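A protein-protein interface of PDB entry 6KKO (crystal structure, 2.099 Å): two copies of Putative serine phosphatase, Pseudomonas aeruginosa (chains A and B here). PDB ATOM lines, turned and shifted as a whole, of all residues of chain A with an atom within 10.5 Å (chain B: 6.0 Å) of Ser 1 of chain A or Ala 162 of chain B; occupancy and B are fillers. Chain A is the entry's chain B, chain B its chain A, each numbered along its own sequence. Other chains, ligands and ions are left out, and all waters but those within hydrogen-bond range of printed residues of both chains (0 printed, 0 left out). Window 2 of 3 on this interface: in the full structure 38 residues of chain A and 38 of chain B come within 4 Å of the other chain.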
ATOM      1  N   SER A   1       5.529  18.460   2.035  1.00  0.00           N
ATOM      2  CA  SER A   1       6.957  18.569   1.761  1.00  0.00           C
ATOM      3  C   SER A   1       7.519  19.858   2.353  1.00  0.00           C
ATOM      4  O   SER A   1       8.638  19.882   2.868  1.00  0.00           O
ATOM      5  CB  SER A   1       7.225  18.517   0.258  1.00  0.00           C
ATOM      6  N   MET A   2       6.732  20.926   2.271  1.00  0.00           N
ATOM      7  CA  MET A   2       7.116  22.216   2.828  1.00  0.00           C
ATOM      8  C   MET A   2       7.245  22.111   4.345  1.00  0.00           C
ATOM      9  O   MET A   2       8.094  22.760   4.957  1.00  0.00           O
ATOM     10  CB  MET A   2       6.096  23.288   2.439  1.00  0.00           C
ATOM     11  CG  MET A   2       6.460  24.703   2.859  1.00  0.00           C
ATOM     12  SD  MET A   2       5.528  26.044   1.785  1.00  0.00           S
ATOM     13  CE  MET A   2       3.713  25.340   1.927  1.00  0.00           C
ATOM     14  N   GLU A   3       6.397  21.273   4.944  1.00  0.00           N
ATOM     15  CA  GLU A   3       6.506  21.003   6.372  1.00  0.00           C
ATOM     16  C   GLU A   3       7.654  20.053   6.689  1.00  0.00           C
ATOM     17  O   GLU A   3       8.258  20.161   7.762  1.00  0.00           O
ATOM     18  CB  GLU A   3       5.192  20.433   6.909  1.00  0.00           C
ATOM     19  CG  GLU A   3       4.093  21.469   7.080  1.00  0.00           C
ATOM     20  CD  GLU A   3       3.408  21.826   5.776  1.00  0.00           C
ATOM     21  OE1 GLU A   3       3.031  20.898   5.028  1.00  0.00           O
ATOM     22  OE2 GLU A   3       3.248  23.034   5.503  1.00  0.00           O
ATOM     23  N   THR A   4       7.969  19.118   5.786  1.00  0.00           N
ATOM     24  CA  THR A   4       9.090  18.218   6.041  1.00  0.00           C
ATOM     25  C   THR A   4      10.422  18.939   5.873  1.00  0.00           C
ATOM     26  O   THR A   4      11.357  18.712   6.649  1.00  0.00           O
ATOM     27  CB  THR A   4       9.021  16.988   5.129  1.00  0.00           C
ATOM     28  OG1 THR A   4       9.098  17.384   3.753  1.00  0.00           O
ATOM     29  CG2 THR A   4       7.733  16.222   5.365  1.00  0.00           C
ATOM     30  N   LEU A   5      10.522  19.822   4.875  1.00  0.00           N
ATOM     31  CA  LEU A   5      11.732  20.624   4.716  1.00  0.00           C
ATOM     32  C   LEU A   5      11.936  21.561   5.902  1.00  0.00           C
ATOM     33  O   LEU A   5      13.059  21.701   6.404  1.00  0.00           O
ATOM     34  CB  LEU A   5      11.673  21.421   3.411  1.00  0.00           C
ATOM     35  CG  LEU A   5      11.747  20.646   2.094  1.00  0.00           C
ATOM     36  CD1 LEU A   5      11.230  21.503   0.952  1.00  0.00           C
ATOM     37  CD2 LEU A   5      13.173  20.195   1.818  1.00  0.00           C
ATOM     38  N   ASP A   6      10.864  22.217   6.359  1.00  0.00           N
ATOM     39  CA  ASP A   6      10.981  23.114   7.507  1.00  0.00           C
ATOM     40  C   ASP A   6      11.325  22.346   8.775  1.00  0.00           C
ATOM     41  O   ASP A   6      12.078  22.842   9.622  1.00  0.00           O
ATOM     42  CB  ASP A   6       9.687  23.904   7.692  1.00  0.00           C
ATOM     43  CG  ASP A   6       9.598  25.101   6.768  1.00  0.00           C
ATOM     44  OD1 ASP A   6      10.664  25.610   6.357  1.00  0.00           O
ATOM     45  OD2 ASP A   6       8.469  25.538   6.460  1.00  0.00           O
ATOM     46  N   LEU A   7      10.777  21.137   8.929  1.00  0.00           N
ATOM     47  CA  LEU A   7      11.198  20.278  10.030  1.00  0.00           C
ATOM     48  C   LEU A   7      12.687  19.979   9.957  1.00  0.00           C
ATOM     49  O   LEU A   7      13.348  19.854  10.994  1.00  0.00           O
ATOM     50  CB  LEU A   7      10.397  18.977  10.017  1.00  0.00           C
ATOM     51  CG  LEU A   7      10.456  18.141  11.296  1.00  0.00           C
ATOM     52  CD1 LEU A   7       9.841  18.895  12.465  1.00  0.00           C
ATOM     53  CD2 LEU A   7       9.768  16.806  11.087  1.00  0.00           C
ATOM     54  N   LEU A   8      13.233  19.863   8.745  1.00  0.00           N
ATOM     55  CA  LEU A   8      14.671  19.661   8.606  1.00  0.00           C
ATOM     56  C   LEU A   8      15.433  20.941   8.927  1.00  0.00           C
ATOM     57  O   LEU A   8      16.488  20.895   9.570  1.00  0.00           O
ATOM     58  CB  LEU A   8      15.005  19.171   7.199  1.00  0.00           C
ATOM     59  CG  LEU A   8      16.501  19.042   6.906  1.00  0.00           C
ATOM     60  CD1 LEU A   8      17.152  18.020   7.833  1.00  0.00           C
ATOM     61  CD2 LEU A   8      16.745  18.702   5.439  1.00  0.00           C
ATOM     62  N   ALA A   9      14.903  22.092   8.504  1.00  0.00           N
ATOM     63  CA  ALA A   9      15.555  23.363   8.802  1.00  0.00           C
ATOM     64  C   ALA A   9      15.598  23.623  10.302  1.00  0.00           C
ATOM     65  O   ALA A   9      16.572  24.185  10.817  1.00  0.00           O
ATOM     66  CB  ALA A   9      14.840  24.505   8.079  1.00  0.00           C
ATOM     67  N   ILE B 115       6.343   5.271   1.409  1.00  0.00           N
ATOM     68  CA  ILE B 115       5.417   6.393   1.515  1.00  0.00           C
ATOM     69  C   ILE B 115       5.037   6.908   0.133  1.00  0.00           C
ATOM     70  O   ILE B 115       3.869   7.230  -0.121  1.00  0.00           O
ATOM     71  CB  ILE B 115       6.017   7.498   2.399  1.00  0.00           C
ATOM     72  CG1 ILE B 115       6.095   7.002   3.843  1.00  0.00           C
ATOM     73  CG2 ILE B 115       5.191   8.766   2.301  1.00  0.00           C
ATOM     74  CD1 ILE B 115       6.833   7.915   4.764  1.00  0.00           C
ATOM     75  N   PRO B 160      -2.028  13.904   0.555  1.00  0.00           N
ATOM     76  CA  PRO B 160      -1.104  12.762   0.509  1.00  0.00           C
ATOM     77  C   PRO B 160       0.035  12.926   1.509  1.00  0.00           C
ATOM     78  O   PRO B 160       0.547  14.029   1.728  1.00  0.00           O
ATOM     79  CB  PRO B 160      -0.596  12.772  -0.937  1.00  0.00           C
ATOM     80  CG  PRO B 160      -1.661  13.484  -1.710  1.00  0.00           C
ATOM     81  CD  PRO B 160      -2.186  14.535  -0.767  1.00  0.00           C
ATOM     82  N   LEU B 161       0.420  11.810   2.128  1.00  0.00           N
ATOM     83  CA  LEU B 161       1.547  11.815   3.052  1.00  0.00           C
ATOM     84  C   LEU B 161       2.808  12.292   2.347  1.00  0.00           C
ATOM     85  O   LEU B 161       3.090  11.901   1.212  1.00  0.00           O
ATOM     86  CB  LEU B 161       1.770  10.413   3.621  1.00  0.00           C
ATOM     87  CG  LEU B 161       1.388  10.170   5.077  1.00  0.00           C
ATOM     88  CD1 LEU B 161      -0.023  10.653   5.354  1.00  0.00           C
ATOM     89  CD2 LEU B 161       1.539   8.690   5.413  1.00  0.00           C
ATOM     90  N   ALA B 162       3.562  13.158   3.018  1.00  0.00           N
ATOM     91  CA  ALA B 162       4.810  13.686   2.489  1.00  0.00           C
ATOM     92  C   ALA B 162       5.964  13.298   3.399  1.00  0.00           C
ATOM     93  O   ALA B 162       5.856  13.371   4.626  1.00  0.00           O
ATOM     94  CB  ALA B 162       4.755  15.212   2.331  1.00  0.00           C
ATOM     95  N   ALA B 163       7.067  12.877   2.789  1.00  0.00           N
ATOM     96  CA  ALA B 163       8.263  12.505   3.523  1.00  0.00           C
ATOM     97  C   ALA B 163       9.474  13.093   2.817  1.00  0.00           C
ATOM     98  O   ALA B 163       9.440  13.391   1.620  1.00  0.00           O
ATOM     99  CB  ALA B 163       8.406  10.979   3.647  1.00  0.00           C
ATOM    100  N   SER B 164      10.548  13.265   3.579  1.00  0.00           N
ATOM    101  CA  SER B 164      11.813  13.715   3.027  1.00  0.00           C
ATOM    102  C   SER B 164      12.926  13.049   3.818  1.00  0.00           C
ATOM    103  O   SER B 164      12.705  12.511   4.908  1.00  0.00           O
ATOM    104  CB  SER B 164      11.955  15.242   3.067  1.00  0.00           C
ATOM    105  OG  SER B 164      11.862  15.740   4.391  1.00  0.00           O
ATOM    106  N   SER B 176      11.962  12.798   7.895  1.00  0.00           N
ATOM    107  CA  SER B 176      10.904  13.676   8.383  1.00  0.00           C
ATOM    108  C   SER B 176       9.619  13.374   7.630  1.00  0.00           C
ATOM    109  O   SER B 176       9.624  13.270   6.400  1.00  0.00           O
ATOM    110  CB  SER B 176      11.283  15.158   8.237  1.00  0.00           C
ATOM    111  OG  SER B 176      11.452  15.523   6.878  1.00  0.00           O
ATOM    112  N   LEU B 177       8.524  13.255   8.374  1.00  0.00           N
ATOM    113  CA  LEU B 177       7.220  12.876   7.852  1.00  0.00           C
ATOM    114  C   LEU B 177       6.194  13.907   8.289  1.00  0.00           C
ATOM    115  O   LEU B 177       6.249  14.397   9.419  1.00  0.00           O
ATOM    116  CB  LEU B 177       6.821  11.483   8.358  1.00  0.00           C
ATOM    117  CG  LEU B 177       5.422  10.945   8.067  1.00  0.00           C
ATOM    118  CD1 LEU B 177       5.259  10.638   6.588  1.00  0.00           C
ATOM    119  CD2 LEU B 177       5.130   9.712   8.924  1.00  0.00           C
ATOM    120  N   ARG B 178       5.260  14.238   7.399  1.00  0.00           N
ATOM    121  CA  ARG B 178       4.209  15.181   7.748  1.00  0.00           C
ATOM    122  C   ARG B 178       2.877  14.687   7.202  1.00  0.00           C
ATOM    123  O   ARG B 178       2.803  14.162   6.083  1.00  0.00           O
ATOM    124  CB  ARG B 178       4.523  16.603   7.236  1.00  0.00           C
ATOM    125  CG  ARG B 178       4.172  16.887   5.784  1.00  0.00           C
ATOM    126  CD  ARG B 178       2.833  17.606   5.661  1.00  0.00           C
ATOM    127  NE  ARG B 178       2.473  17.849   4.268  1.00  0.00           N
ATOM    128  CZ  ARG B 178       1.878  16.955   3.482  1.00  0.00           C
ATOM    129  NH1 ARG B 178       1.573  15.751   3.949  1.00  0.00           N
ATOM    130  NH2 ARG B 178       1.590  17.266   2.226  1.00  0.00           N
ATOM    131  N   ALA B 179       1.837  14.834   8.016  1.00  0.00           N
ATOM    132  CA  ALA B 179       0.470  14.515   7.640  1.00  0.00           C
ATOM    133  C   ALA B 179      -0.388  15.759   7.809  1.00  0.00           C
ATOM    134  O   ALA B 179      -0.197  16.534   8.752  1.00  0.00           O
ATOM    135  CB  ALA B 179      -0.098  13.375   8.491  1.00  0.00           C
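OG of Ser 164 of chain B sits close to OG1 of Thr 4 of chain A (3.3 Å). The side-chain hydroxyl of Ser 176 of chain B is in hydrogen-bond range of the backbone carbonyl oxygen of Thr 4 of chain A (3.2 Å). The guanidinium group (NE) of Arg 178 of chain B is in salt-bridge range of the side-chain carboxylate (OE1) of Glu 3 of chain A (3.2 Å).
The guanidinium group of Arg 178 of chain B sits at hydrogen-bond distance from the backbone carbonyl oxygen of Pro 160 of chain B (3.0 Å). The backbone carbonyl oxygen (O) of Ala 162 of chain B lies within hydrogen-bond range of the backbone NH (N) of Arg 178 of chain B (3.0 Å). The side-chain hydroxyl of Ser 164 of chain B lies within hydrogen-bond range of the side-chain hydroxyl of Ser 176 of chain B (2.5 Å). The backbone carbonyl oxygen (O) of Ser 1 of chain A is in hydrogen-bond range of the side-chain hydroxyl (OG1) of Thr 4 of chain A (2.7 Å).
Among the printed residues, merely in contact across the chains: Ser 1 of chain A with Ala 162 of chain B, Thr 4 of chain A with Ala 162 of chain B, Leu 7 of chain A with Ser 176 of chain B, Thr 4 of chain A with Arg 178 of chain B and Ser 1 of chain A with Arg 178 of chain B.
Of chain B, only Ala 162 (3.4 Å) and Arg 178 (3.8 Å) come within 4 Å of Ser 1 of chain A. Of the printed residues of chain B, Glu 3 of chain A touches Arg 178. Printed residues of chain B within 4 Å of Thr 4 of chain A: Ala 162, Ser 164, Ser 176 and Arg 178. Of the printed residues of chain B, Leu 7 of chain A touches Ser 176. No residue of chain A comes within 4 Å of Leu 161 of chain B. Of chain A, only Ser 1 and Thr 4 come within 4 Å of Ala 162 of chain B. Of the printed residues of chain A, Ser 164 of chain B touches Thr 4 (3.2 Å). Of the printed residues of chain A, Ser 176 of chain B touches Thr 4 and Leu 7. No residue of chain A comes within 4 Å of Leu 177 of chain B. Arg 178 of chain B touches just these residues of chain A: Ser 1 (3.8 Å), Glu 3 (3.2 Å) and Thr 4 (3.6 Å).
Of the 10 printed residues of chain B, 4 touch a printed residue of chain A. Printed residues of chain B that touch a printed residue of chain A: Ala 162, Ser 164, Ser 176 and Arg 178. Hydrophobic or aromatic side chains of chain A that line the printed part of chain B: Leu 7. Among the printed residues, Asp or Glu carboxylates within 4 Å of a Lys or Arg side-chain nitrogen of the other chain: Glu 3 of chain A with Arg 178 of chain B (3.2 Å).
No position is printed for both chains. Of the 8 pairs that touch across the chains among the printed residues, none has its exchanged pair printed and touching as well.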
